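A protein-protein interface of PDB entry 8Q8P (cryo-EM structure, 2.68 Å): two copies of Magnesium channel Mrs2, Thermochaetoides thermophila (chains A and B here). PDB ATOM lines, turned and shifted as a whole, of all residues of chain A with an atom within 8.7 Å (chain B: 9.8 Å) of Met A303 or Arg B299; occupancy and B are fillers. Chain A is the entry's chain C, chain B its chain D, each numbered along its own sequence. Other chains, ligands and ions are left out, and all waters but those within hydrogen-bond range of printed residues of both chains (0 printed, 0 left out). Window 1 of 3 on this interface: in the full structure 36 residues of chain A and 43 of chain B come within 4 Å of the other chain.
Of the 18 printed residues of chain B, 8 touch a printed residue of chain A. Of the 18 printed residues of chain A, 7 touch a printed residue of chain B. Hydrophobic or aromatic side chains of chain A within 4 Å of the printed part of chain B: Met A303 and Leu A307. Among the printed residues, Asp or Glu carboxylates within 4 Å of a Lys or Arg side-chain nitrogen of the other chain: Asp A296 with Arg B292 and Arg A299 with Asp B296.
NH2 of Arg A292 is in salt-bridge range of OD2 of Asp A296. The guanidinium group of Arg A299 is in salt-bridge range of the side-chain carboxylate of Asp A296 (3.8 Å). The guanidinium group (NH1) of Arg A299 lies within hydrogen-bond range of the side-chain amide oxygen (OD1) of Asn A300. O of Asp A306 sits at hydrogen-bond distance from OG of Ser A310 (3.1 Å). The side-chain carboxylate (OD2) of Asp B296 lies within salt-bridge range of the guanidinium group (NH2) of Arg B299 (3.8 Å). OG of Ser B301 sits at hydrogen-bond distance from O of Asn B298, at 2.7 Å.
Arg A292 touches its own counterpart, Arg B292. Asp A296 touches its own counterpart, Asp B296. Arg B299 touches its own counterpart, Arg A299. Met B303 touches its own counterpart, Met A303. 13 positions are printed for both chains.
The guanidinium group of Arg B292 is in salt-bridge range of the side-chain carboxylate of Asp A296, at 3.9 Å. The side-chain carboxylate (OD1) of Asp B296 is in salt-bridge range of the guanidinium group (NH2) of Arg A299, at 3.5 Å. The side-chain amide nitrogen (ND2) of Asn A300 lies close to the side-chain amide nitrogen (ND2) of Asn B298. NH1 of Arg B292 sits close to NH2 of Arg A292, 3.0 Å away.
Met A303 touches just these residues of chain B: Arg B299 and Met B303. Arg B299 touches just these residues of chain A: Arg A299 and Met A303. Ser A301 touches none of the printed residues of chain B. No residue of chain B comes within 4 Å of Leu A302. Asn B300 touches none of the printed residues of chain A. Of the printed residues of chain A, Met B303 touches Met A303. Of the printed residues of chain B, Ser A310 touches Asp B306 (3.6 Å). Leu B305 touches none of the printed residues of chain A. The nearest residue of chain B that does not touch Met A303 is Leu B302 (4.4 Å).
Asp A296 touches Leu B295 (CB to CD1, 3.98 Å). Asp A296 touches Asp B296 (OD2 to OD1, 3.7 Å). Arg B299 touches Arg A299 (CB to NH1, 3.3 Å). Met A303 touches Arg B299. Met A303 touches Met B303. Leu A307 touches Leu B302 (CD1 to CD2, 3.95 Å). Asp B306 touches Leu A307 (OD1 to CD2, 3.4 Å). Ser A310 touches Asp B306.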
ATOM      1  N   ARG A 292      -4.511   2.038 -19.590  1.00  0.00           N
ATOM      2  CA  ARG A 292      -5.652   2.774 -20.125  1.00  0.00           C
ATOM      3  C   ARG A 292      -6.777   1.838 -20.546  1.00  0.00           C
ATOM      4  O   ARG A 292      -7.954   2.134 -20.307  1.00  0.00           O
ATOM      5  CB  ARG A 292      -5.219   3.630 -21.314  1.00  0.00           C
ATOM      6  CG  ARG A 292      -6.180   4.760 -21.634  1.00  0.00           C
ATOM      7  CD  ARG A 292      -6.617   4.720 -23.088  1.00  0.00           C
ATOM      8  NE  ARG A 292      -7.531   3.609 -23.331  1.00  0.00           N
ATOM      9  CZ  ARG A 292      -8.843   3.668 -23.150  1.00  0.00           C
ATOM     10  NH1 ARG A 292      -9.438   4.780 -22.751  1.00  0.00           N
ATOM     11  NH2 ARG A 292      -9.578   2.582 -23.373  1.00  0.00           N
ATOM     12  N   ASP A 296     -10.994   0.419 -18.647  1.00  0.00           N
ATOM     13  CA  ASP A 296     -12.256   0.134 -19.321  1.00  0.00           C
ATOM     14  C   ASP A 296     -12.606  -1.346 -19.252  1.00  0.00           C
ATOM     15  O   ASP A 296     -13.790  -1.701 -19.251  1.00  0.00           O
ATOM     16  CB  ASP A 296     -12.194   0.598 -20.775  1.00  0.00           C
ATOM     17  CG  ASP A 296     -11.992   2.095 -20.900  1.00  0.00           C
ATOM     18  OD1 ASP A 296     -11.881   2.772 -19.857  1.00  0.00           O
ATOM     19  OD2 ASP A 296     -11.946   2.596 -22.044  1.00  0.00           O
ATOM     20  N   ALA A 297     -11.598  -2.219 -19.198  1.00  0.00           N
ATOM     21  CA  ALA A 297     -11.871  -3.645 -19.063  1.00  0.00           C
ATOM     22  C   ALA A 297     -12.518  -3.960 -17.720  1.00  0.00           C
ATOM     23  O   ALA A 297     -13.448  -4.772 -17.650  1.00  0.00           O
ATOM     24  CB  ALA A 297     -10.582  -4.446 -19.240  1.00  0.00           C
ATOM     25  N   ASN A 298     -12.042  -3.335 -16.644  1.00  0.00           N
ATOM     26  CA  ASN A 298     -12.594  -3.626 -15.324  1.00  0.00           C
ATOM     27  C   ASN A 298     -13.858  -2.832 -15.008  1.00  0.00           C
ATOM     28  O   ASN A 298     -14.565  -3.185 -14.058  1.00  0.00           O
ATOM     29  CB  ASN A 298     -11.541  -3.386 -14.230  1.00  0.00           C
ATOM     30  CG  ASN A 298     -11.422  -1.927 -13.827  1.00  0.00           C
ATOM     31  OD1 ASN A 298     -10.598  -1.192 -14.363  1.00  0.00           O
ATOM     32  ND2 ASN A 298     -12.230  -1.508 -12.858  1.00  0.00           N
ATOM     33  N   ARG A 299     -14.165  -1.779 -15.771  1.00  0.00           N
ATOM     34  CA  ARG A 299     -15.417  -1.056 -15.542  1.00  0.00           C
ATOM     35  C   ARG A 299     -16.635  -1.887 -15.955  1.00  0.00           C
ATOM     36  O   ARG A 299     -17.702  -1.808 -15.320  1.00  0.00           O
ATOM     37  CB  ARG A 299     -15.380   0.280 -16.288  1.00  0.00           C
ATOM     38  CG  ARG A 299     -16.733   0.929 -16.537  1.00  0.00           C
ATOM     39  CD  ARG A 299     -17.187   0.720 -17.971  1.00  0.00           C
ATOM     40  NE  ARG A 299     -16.340   1.430 -18.920  1.00  0.00           N
ATOM     41  CZ  ARG A 299     -16.352   1.230 -20.231  1.00  0.00           C
ATOM     42  NH1 ARG A 299     -17.148   0.331 -20.784  1.00  0.00           N
ATOM     43  NH2 ARG A 299     -15.542   1.947 -21.004  1.00  0.00           N
ATOM     44  N   ASN A 300     -16.493  -2.691 -17.012  1.00  0.00           N
ATOM     45  CA  ASN A 300     -17.626  -3.456 -17.526  1.00  0.00           C
ATOM     46  C   ASN A 300     -18.143  -4.468 -16.511  1.00  0.00           C
ATOM     47  O   ASN A 300     -19.321  -4.833 -16.557  1.00  0.00           O
ATOM     48  CB  ASN A 300     -17.242  -4.158 -18.827  1.00  0.00           C
ATOM     49  CG  ASN A 300     -17.180  -3.208 -20.009  1.00  0.00           C
ATOM     50  OD1 ASN A 300     -17.054  -1.995 -19.839  1.00  0.00           O
ATOM     51  ND2 ASN A 300     -17.273  -3.755 -21.215  1.00  0.00           N
ATOM     52  N   SER A 301     -17.293  -4.921 -15.586  1.00  0.00           N
ATOM     53  CA  SER A 301     -17.755  -5.856 -14.565  1.00  0.00           C
ATOM     54  C   SER A 301     -18.820  -5.225 -13.677  1.00  0.00           C
ATOM     55  O   SER A 301     -19.885  -5.815 -13.458  1.00  0.00           O
ATOM     56  CB  SER A 301     -16.573  -6.342 -13.727  1.00  0.00           C
ATOM     57  OG  SER A 301     -15.924  -5.261 -13.083  1.00  0.00           O
ATOM     58  N   LEU A 302     -18.559  -4.019 -13.167  1.00  0.00           N
ATOM     59  CA  LEU A 302     -19.566  -3.315 -12.379  1.00  0.00           C
ATOM     60  C   LEU A 302     -20.770  -2.940 -13.234  1.00  0.00           C
ATOM     61  O   LEU A 302     -21.919  -3.004 -12.768  1.00  0.00           O
ATOM     62  CB  LEU A 302     -18.953  -2.070 -11.738  1.00  0.00           C
ATOM     63  CG  LEU A 302     -17.669  -2.273 -10.930  1.00  0.00           C
ATOM     64  CD1 LEU A 302     -17.135  -0.939 -10.431  1.00  0.00           C
ATOM     65  CD2 LEU A 302     -17.902  -3.227  -9.770  1.00  0.00           C
ATOM     66  N   MET A 303     -20.524  -2.537 -14.487  1.00  0.00           N
ATOM     67  CA  MET A 303     -21.636  -2.192 -15.371  1.00  0.00           C
ATOM     68  C   MET A 303     -22.589  -3.370 -15.549  1.00  0.00           C
ATOM     69  O   MET A 303     -23.811  -3.190 -15.588  1.00  0.00           O
ATOM     70  CB  MET A 303     -21.112  -1.719 -16.726  1.00  0.00           C
ATOM     71  CG  MET A 303     -20.712  -0.257 -16.755  1.00  0.00           C
ATOM     72  SD  MET A 303     -20.696   0.409 -18.428  1.00  0.00           S
ATOM     73  CE  MET A 303     -22.348  -0.018 -18.969  1.00  0.00           C
ATOM     74  N   LEU A 304     -22.047  -4.585 -15.662  1.00  0.00           N
ATOM     75  CA  LEU A 304     -22.882  -5.774 -15.786  1.00  0.00           C
ATOM     76  C   LEU A 304     -23.498  -6.184 -14.455  1.00  0.00           C
ATOM     77  O   LEU A 304     -24.624  -6.696 -14.430  1.00  0.00           O
ATOM     78  CB  LEU A 304     -22.060  -6.929 -16.364  1.00  0.00           C
ATOM     79  CG  LEU A 304     -22.753  -8.283 -16.516  1.00  0.00           C
ATOM     80  CD1 LEU A 304     -23.825  -8.229 -17.595  1.00  0.00           C
ATOM     81  CD2 LEU A 304     -21.736  -9.373 -16.816  1.00  0.00           C
ATOM     82  N   LEU A 305     -22.786  -5.970 -13.346  1.00  0.00           N
ATOM     83  CA  LEU A 305     -23.319  -6.349 -12.041  1.00  0.00           C
ATOM     84  C   LEU A 305     -24.525  -5.502 -11.652  1.00  0.00           C
ATOM     85  O   LEU A 305     -25.422  -5.992 -10.957  1.00  0.00           O
ATOM     86  CB  LEU A 305     -22.227  -6.237 -10.977  1.00  0.00           C
ATOM     87  CG  LEU A 305     -22.600  -6.664  -9.556  1.00  0.00           C
ATOM     88  CD1 LEU A 305     -23.023  -8.124  -9.524  1.00  0.00           C
ATOM     89  CD2 LEU A 305     -21.446  -6.417  -8.598  1.00  0.00           C
ATOM     90  N   ASP A 306     -24.565  -4.238 -12.083  1.00  0.00           N
ATOM     91  CA  ASP A 306     -25.696  -3.380 -11.725  1.00  0.00           C
ATOM     92  C   ASP A 306     -27.016  -3.888 -12.306  1.00  0.00           C
ATOM     93  O   ASP A 306     -28.082  -3.685 -11.704  1.00  0.00           O
ATOM     94  CB  ASP A 306     -25.432  -1.947 -12.188  1.00  0.00           C
ATOM     95  CG  ASP A 306     -26.520  -0.984 -11.755  1.00  0.00           C
ATOM     96  OD1 ASP A 306     -26.588  -0.664 -10.549  1.00  0.00           O
ATOM     97  OD2 ASP A 306     -27.308  -0.546 -12.619  1.00  0.00           O
ATOM     98  N   LEU A 307     -26.969  -4.549 -13.467  1.00  0.00           N
ATOM     99  CA  LEU A 307     -28.197  -4.969 -14.136  1.00  0.00           C
ATOM    100  C   LEU A 307     -28.938  -6.051 -13.359  1.00  0.00           C
ATOM    101  O   LEU A 307     -30.172  -6.100 -13.397  1.00  0.00           O
ATOM    102  CB  LEU A 307     -27.884  -5.450 -15.552  1.00  0.00           C
ATOM    103  CG  LEU A 307     -27.516  -4.350 -16.550  1.00  0.00           C
ATOM    104  CD1 LEU A 307     -27.102  -4.937 -17.889  1.00  0.00           C
ATOM    105  CD2 LEU A 307     -28.678  -3.388 -16.728  1.00  0.00           C
ATOM    106  N   LYS A 308     -28.215  -6.927 -12.657  1.00  0.00           N
ATOM    107  CA  LYS A 308     -28.883  -7.945 -11.850  1.00  0.00           C
ATOM    108  C   LYS A 308     -29.687  -7.313 -10.720  1.00  0.00           C
ATOM    109  O   LYS A 308     -30.826  -7.717 -10.455  1.00  0.00           O
ATOM    110  CB  LYS A 308     -27.856  -8.932 -11.298  1.00  0.00           C
ATOM    111  CG  LYS A 308     -27.042  -9.637 -12.371  1.00  0.00           C
ATOM    112  CD  LYS A 308     -26.012 -10.568 -11.757  1.00  0.00           C
ATOM    113  CE  LYS A 308     -25.178 -11.251 -12.828  1.00  0.00           C
ATOM    114  NZ  LYS A 308     -24.137 -12.134 -12.233  1.00  0.00           N
ATOM    115  N   PHE A 309     -29.112  -6.312 -10.050  1.00  0.00           N
ATOM    116  CA  PHE A 309     -29.853  -5.588  -9.023  1.00  0.00           C
ATOM    117  C   PHE A 309     -31.042  -4.850  -9.623  1.00  0.00           C
ATOM    118  O   PHE A 309     -32.115  -4.781  -9.010  1.00  0.00           O
ATOM    119  CB  PHE A 309     -28.926  -4.616  -8.294  1.00  0.00           C
ATOM    120  CG  PHE A 309     -27.813  -5.288  -7.542  1.00  0.00           C
ATOM    121  CD1 PHE A 309     -26.586  -4.664  -7.392  1.00  0.00           C
ATOM    122  CD2 PHE A 309     -27.995  -6.541  -6.981  1.00  0.00           C
ATOM    123  CE1 PHE A 309     -25.560  -5.280  -6.700  1.00  0.00           C
ATOM    124  CE2 PHE A 309     -26.973  -7.161  -6.288  1.00  0.00           C
ATOM    125  CZ  PHE A 309     -25.754  -6.530  -6.147  1.00  0.00           C
ATOM    126  N   SER A 310     -30.872  -4.286 -10.823  1.00  0.00           N
ATOM    127  CA  SER A 310     -31.995  -3.627 -11.485  1.00  0.00           C
ATOM    128  C   SER A 310     -33.134  -4.608 -11.751  1.00  0.00           C
ATOM    129  O   SER A 310     -34.309  -4.291 -11.524  1.00  0.00           O
ATOM    130  CB  SER A 310     -31.531  -2.975 -12.786  1.00  0.00           C
ATOM    131  OG  SER A 310     -30.543  -1.991 -12.539  1.00  0.00           O
ATOM    132  N   LEU A 363     -30.854 -10.903 -20.174  1.00  0.00           N
ATOM    133  CA  LEU A 363     -29.514 -10.376 -19.930  1.00  0.00           C
ATOM    134  C   LEU A 363     -28.442 -11.349 -20.403  1.00  0.00           C
ATOM    135  O   LEU A 363     -27.446 -10.939 -21.011  1.00  0.00           O
ATOM    136  CB  LEU A 363     -29.337 -10.063 -18.445  1.00  0.00           C
ATOM    137  CG  LEU A 363     -27.926  -9.682 -17.995  1.00  0.00           C
ATOM    138  CD1 LEU A 363     -27.428  -8.467 -18.761  1.00  0.00           C
ATOM    139  CD2 LEU A 363     -27.890  -9.424 -16.497  1.00  0.00           C
ATOM    140  N   VAL A 366     -28.283 -11.224 -24.164  1.00  0.00           N
ATOM    141  CA  VAL A 366     -27.665 -10.000 -24.667  1.00  0.00           C
ATOM    142  C   VAL A 366     -26.153 -10.040 -24.471  1.00  0.00           C
ATOM    143  O   VAL A 366     -25.384  -9.727 -25.387  1.00  0.00           O
ATOM    144  CB  VAL A 366     -28.290  -8.765 -23.993  1.00  0.00           C
ATOM    145  CG1 VAL A 366     -27.452  -7.527 -24.268  1.00  0.00           C
ATOM    146  CG2 VAL A 366     -29.715  -8.560 -24.484  1.00  0.00           C
ATOM    147  N   ILE B 198     -12.209 -10.328 -24.457  1.00  0.00           N
ATOM    148  CA  ILE B 198     -11.212  -9.523 -23.761  1.00  0.00           C
ATOM    149  C   ILE B 198     -11.363  -9.789 -22.269  1.00  0.00           C
ATOM    150  O   ILE B 198     -12.369  -9.402 -21.661  1.00  0.00           O
ATOM    151  CB  ILE B 198     -11.363  -8.028 -24.069  1.00  0.00           C
ATOM    152  CG1 ILE B 198     -11.335  -7.792 -25.581  1.00  0.00           C
ATOM    153  CG2 ILE B 198     -10.269  -7.230 -23.380  1.00  0.00           C
ATOM    154  CD1 ILE B 198     -11.628  -6.365 -25.978  1.00  0.00           C
ATOM    155  N   ILE B 291      -9.136  -3.475 -30.136  1.00  0.00           N
ATOM    156  CA  ILE B 291      -9.858  -3.930 -28.948  1.00  0.00           C
ATOM    157  C   ILE B 291     -10.258  -2.748 -28.069  1.00  0.00           C
ATOM    158  O   ILE B 291     -11.291  -2.796 -27.378  1.00  0.00           O
ATOM    159  CB  ILE B 291      -9.032  -4.969 -28.166  1.00  0.00           C
ATOM    160  CG1 ILE B 291      -7.727  -4.360 -27.650  1.00  0.00           C
ATOM    161  CG2 ILE B 291      -8.756  -6.193 -29.028  1.00  0.00           C
ATOM    162  CD1 ILE B 291      -6.862  -5.335 -26.882  1.00  0.00           C
ATOM    163  N   ARG B 292      -9.471  -1.664 -28.094  1.00  0.00           N
ATOM    164  CA  ARG B 292      -9.831  -0.478 -27.324  1.00  0.00           C
ATOM    165  C   ARG B 292     -11.194   0.066 -27.735  1.00  0.00           C
ATOM    166  O   ARG B 292     -11.983   0.475 -26.876  1.00  0.00           O
ATOM    167  CB  ARG B 292      -8.768   0.606 -27.492  1.00  0.00           C
ATOM    168  CG  ARG B 292      -8.793   1.660 -26.400  1.00  0.00           C
ATOM    169  CD  ARG B 292      -8.898   3.058 -26.982  1.00  0.00           C
ATOM    170  NE  ARG B 292     -10.229   3.305 -27.523  1.00  0.00           N
ATOM    171  CZ  ARG B 292     -11.256   3.746 -26.811  1.00  0.00           C
ATOM    172  NH1 ARG B 292     -11.134   4.029 -25.524  1.00  0.00           N
ATOM    173  NH2 ARG B 292     -12.437   3.904 -27.401  1.00  0.00           N
ATOM    174  N   ALA B 293     -11.490   0.074 -29.034  1.00  0.00           N
ATOM    175  CA  ALA B 293     -12.797   0.504 -29.514  1.00  0.00           C
ATOM    176  C   ALA B 293     -13.852  -0.582 -29.376  1.00  0.00           C
ATOM    177  O   ALA B 293     -15.039  -0.265 -29.231  1.00  0.00           O
ATOM    178  CB  ALA B 293     -12.706   0.946 -30.977  1.00  0.00           C
ATOM    179  N   ILE B 294     -13.446  -1.854 -29.425  1.00  0.00           N
ATOM    180  CA  ILE B 294     -14.392  -2.950 -29.221  1.00  0.00           C
ATOM    181  C   ILE B 294     -15.030  -2.858 -27.839  1.00  0.00           C
ATOM    182  O   ILE B 294     -16.231  -3.123 -27.669  1.00  0.00           O
ATOM    183  CB  ILE B 294     -13.689  -4.304 -29.437  1.00  0.00           C
ATOM    184  CG1 ILE B 294     -13.551  -4.603 -30.930  1.00  0.00           C
ATOM    185  CG2 ILE B 294     -14.438  -5.429 -28.735  1.00  0.00           C
ATOM    186  CD1 ILE B 294     -14.865  -4.916 -31.613  1.00  0.00           C
ATOM    187  N   LEU B 295     -14.236  -2.490 -26.828  1.00  0.00           N
ATOM    188  CA  LEU B 295     -14.777  -2.356 -25.475  1.00  0.00           C
ATOM    189  C   LEU B 295     -15.922  -1.345 -25.428  1.00  0.00           C
ATOM    190  O   LEU B 295     -17.017  -1.641 -24.925  1.00  0.00           O
ATOM    191  CB  LEU B 295     -13.667  -1.957 -24.503  1.00  0.00           C
ATOM    192  CG  LEU B 295     -12.661  -3.048 -24.133  1.00  0.00           C
ATOM    193  CD1 LEU B 295     -11.587  -2.498 -23.209  1.00  0.00           C
ATOM    194  CD2 LEU B 295     -13.369  -4.229 -23.489  1.00  0.00           C
ATOM    195  N   ASP B 296     -15.685  -0.139 -25.952  1.00  0.00           N
ATOM    196  CA  ASP B 296     -16.723   0.886 -25.952  1.00  0.00           C
ATOM    197  C   ASP B 296     -17.889   0.505 -26.853  1.00  0.00           C
ATOM    198  O   ASP B 296     -19.028   0.907 -26.594  1.00  0.00           O
ATOM    199  CB  ASP B 296     -16.136   2.230 -26.382  1.00  0.00           C
ATOM    200  CG  ASP B 296     -15.066   2.729 -25.431  1.00  0.00           C
ATOM    201  OD1 ASP B 296     -14.766   2.022 -24.446  1.00  0.00           O
ATOM    202  OD2 ASP B 296     -14.525   3.830 -25.668  1.00  0.00           O
ATOM    203  N   ALA B 297     -17.626  -0.263 -27.914  1.00  0.00           N
ATOM    204  CA  ALA B 297     -18.711  -0.716 -28.776  1.00  0.00           C
ATOM    205  C   ALA B 297     -19.648  -1.662 -28.035  1.00  0.00           C
ATOM    206  O   ALA B 297     -20.872  -1.575 -28.189  1.00  0.00           O
ATOM    207  CB  ALA B 297     -18.144  -1.389 -30.024  1.00  0.00           C
ATOM    208  N   ASN B 298     -19.099  -2.572 -27.231  1.00  0.00           N
ATOM    209  CA  ASN B 298     -19.943  -3.531 -26.527  1.00  0.00           C
ATOM    210  C   ASN B 298     -20.519  -2.989 -25.224  1.00  0.00           C
ATOM    211  O   ASN B 298     -21.456  -3.590 -24.686  1.00  0.00           O
ATOM    212  CB  ASN B 298     -19.173  -4.834 -26.253  1.00  0.00           C
ATOM    213  CG  ASN B 298     -18.287  -4.754 -25.023  1.00  0.00           C
ATOM    214  OD1 ASN B 298     -17.107  -4.429 -25.119  1.00  0.00           O
ATOM    215  ND2 ASN B 298     -18.847  -5.079 -23.862  1.00  0.00           N
ATOM    216  N   ARG B 299     -19.997  -1.874 -24.704  1.00  0.00           N
ATOM    217  CA  ARG B 299     -20.591  -1.285 -23.502  1.00  0.00           C
ATOM    218  C   ARG B 299     -21.965  -0.673 -23.790  1.00  0.00           C
ATOM    219  O   ARG B 299     -22.869  -0.715 -22.937  1.00  0.00           O
ATOM    220  CB  ARG B 299     -19.635  -0.245 -22.915  1.00  0.00           C
ATOM    221  CG  ARG B 299     -20.266   0.764 -21.969  1.00  0.00           C
ATOM    222  CD  ARG B 299     -20.487   2.100 -22.659  1.00  0.00           C
ATOM    223  NE  ARG B 299     -19.228   2.755 -22.993  1.00  0.00           N
ATOM    224  CZ  ARG B 299     -19.119   3.795 -23.807  1.00  0.00           C
ATOM    225  NH1 ARG B 299     -20.177   4.319 -24.403  1.00  0.00           N
ATOM    226  NH2 ARG B 299     -17.918   4.322 -24.030  1.00  0.00           N
ATOM    227  N   ASN B 300     -22.141  -0.108 -24.987  1.00  0.00           N
ATOM    228  CA  ASN B 300     -23.389   0.573 -25.315  1.00  0.00           C
ATOM    229  C   ASN B 300     -24.579  -0.378 -25.315  1.00  0.00           C
ATOM    230  O   ASN B 300     -25.711   0.058 -25.090  1.00  0.00           O
ATOM    231  CB  ASN B 300     -23.269   1.271 -26.669  1.00  0.00           C
ATOM    232  CG  ASN B 300     -22.443   2.543 -26.601  1.00  0.00           C
ATOM    233  OD1 ASN B 300     -21.655   2.735 -25.676  1.00  0.00           O
ATOM    234  ND2 ASN B 300     -22.624   3.419 -27.582  1.00  0.00           N
ATOM    235  N   SER B 301     -24.349  -1.673 -25.549  1.00  0.00           N
ATOM    236  CA  SER B 301     -25.451  -2.629 -25.512  1.00  0.00           C
ATOM    237  C   SER B 301     -26.072  -2.705 -24.123  1.00  0.00           C
ATOM    238  O   SER B 301     -27.297  -2.614 -23.977  1.00  0.00           O
ATOM    239  CB  SER B 301     -24.965  -4.007 -25.962  1.00  0.00           C
ATOM    240  OG  SER B 301     -23.930  -4.482 -25.119  1.00  0.00           O
ATOM    241  N   LEU B 302     -25.244  -2.859 -23.087  1.00  0.00           N
ATOM    242  CA  LEU B 302     -25.757  -2.854 -21.720  1.00  0.00           C
ATOM    243  C   LEU B 302     -26.324  -1.488 -21.353  1.00  0.00           C
ATOM    244  O   LEU B 302     -27.349  -1.396 -20.656  1.00  0.00           O
ATOM    245  CB  LEU B 302     -24.654  -3.258 -20.744  1.00  0.00           C
ATOM    246  CG  LEU B 302     -23.914  -4.563 -21.045  1.00  0.00           C
ATOM    247  CD1 LEU B 302     -22.794  -4.787 -20.042  1.00  0.00           C
ATOM    248  CD2 LEU B 302     -24.874  -5.742 -21.051  1.00  0.00           C
ATOM    249  N   MET B 303     -25.665  -0.413 -21.806  1.00  0.00           N
ATOM    250  CA  MET B 303     -26.174   0.926 -21.516  1.00  0.00           C
ATOM    251  C   MET B 303     -27.587   1.114 -22.056  1.00  0.00           C
ATOM    252  O   MET B 303     -28.431   1.739 -21.405  1.00  0.00           O
ATOM    253  CB  MET B 303     -25.237   1.986 -22.091  1.00  0.00           C
ATOM    254  CG  MET B 303     -24.049   2.308 -21.204  1.00  0.00           C
ATOM    255  SD  MET B 303     -23.339   3.919 -21.578  1.00  0.00           S
ATOM    256  CE  MET B 303     -24.790   4.958 -21.443  1.00  0.00           C
ATOM    257  N   LEU B 304     -27.863   0.580 -23.247  1.00  0.00           N
ATOM    258  CA  LEU B 304     -29.201   0.666 -23.821  1.00  0.00           C
ATOM    259  C   LEU B 304     -30.169  -0.314 -23.170  1.00  0.00           C
ATOM    260  O   LEU B 304     -31.360  -0.007 -23.038  1.00  0.00           O
ATOM    261  CB  LEU B 304     -29.138   0.419 -25.330  1.00  0.00           C
ATOM    262  CG  LEU B 304     -30.459   0.414 -26.102  1.00  0.00           C
ATOM    263  CD1 LEU B 304     -31.070   1.805 -26.143  1.00  0.00           C
ATOM    264  CD2 LEU B 304     -30.253  -0.131 -27.507  1.00  0.00           C
ATOM    265  N   LEU B 305     -29.684  -1.488 -22.758  1.00  0.00           N
ATOM    266  CA  LEU B 305     -30.563  -2.472 -22.133  1.00  0.00           C
ATOM    267  C   LEU B 305     -31.076  -1.997 -20.779  1.00  0.00           C
ATOM    268  O   LEU B 305     -32.197  -2.346 -20.389  1.00  0.00           O
ATOM    269  CB  LEU B 305     -29.833  -3.807 -21.986  1.00  0.00           C
ATOM    270  CG  LEU B 305     -30.636  -4.974 -21.409  1.00  0.00           C
ATOM    271  CD1 LEU B 305     -31.840  -5.286 -22.284  1.00  0.00           C
ATOM    272  CD2 LEU B 305     -29.758  -6.203 -21.243  1.00  0.00           C
ATOM    273  N   ASP B 306     -30.279  -1.211 -20.050  1.00  0.00           N
ATOM    274  CA  ASP B 306     -30.722  -0.740 -18.736  1.00  0.00           C
ATOM    275  C   ASP B 306     -31.953   0.162 -18.828  1.00  0.00           C
ATOM    276  O   ASP B 306     -32.777   0.188 -17.900  1.00  0.00           O
ATOM    277  CB  ASP B 306     -29.580  -0.006 -18.032  1.00  0.00           C
ATOM    278  CG  ASP B 306     -29.940   0.418 -16.622  1.00  0.00           C
ATOM    279  OD1 ASP B 306     -30.021  -0.463 -15.739  1.00  0.00           O
ATOM    280  OD2 ASP B 306     -30.141   1.628 -16.394  1.00  0.00           O
ATOM    281  N   PHE B 309     -35.444  -1.596 -18.536  1.00  0.00           N
ATOM    282  CA  PHE B 309     -35.781  -1.901 -17.150  1.00  0.00           C
ATOM    283  C   PHE B 309     -36.166  -0.639 -16.391  1.00  0.00           C
ATOM    284  O   PHE B 309     -37.077  -0.662 -15.552  1.00  0.00           O
ATOM    285  CB  PHE B 309     -34.609  -2.605 -16.468  1.00  0.00           C
ATOM    286  CG  PHE B 309     -34.272  -3.941 -17.068  1.00  0.00           C
ATOM    287  CD1 PHE B 309     -32.966  -4.403 -17.071  1.00  0.00           C
ATOM    288  CD2 PHE B 309     -35.259  -4.735 -17.625  1.00  0.00           C
ATOM    289  CE1 PHE B 309     -32.652  -5.630 -17.622  1.00  0.00           C
ATOM    290  CE2 PHE B 309     -34.951  -5.964 -18.176  1.00  0.00           C
ATOM    291  CZ  PHE B 309     -33.646  -6.412 -18.175  1.00  0.00           C
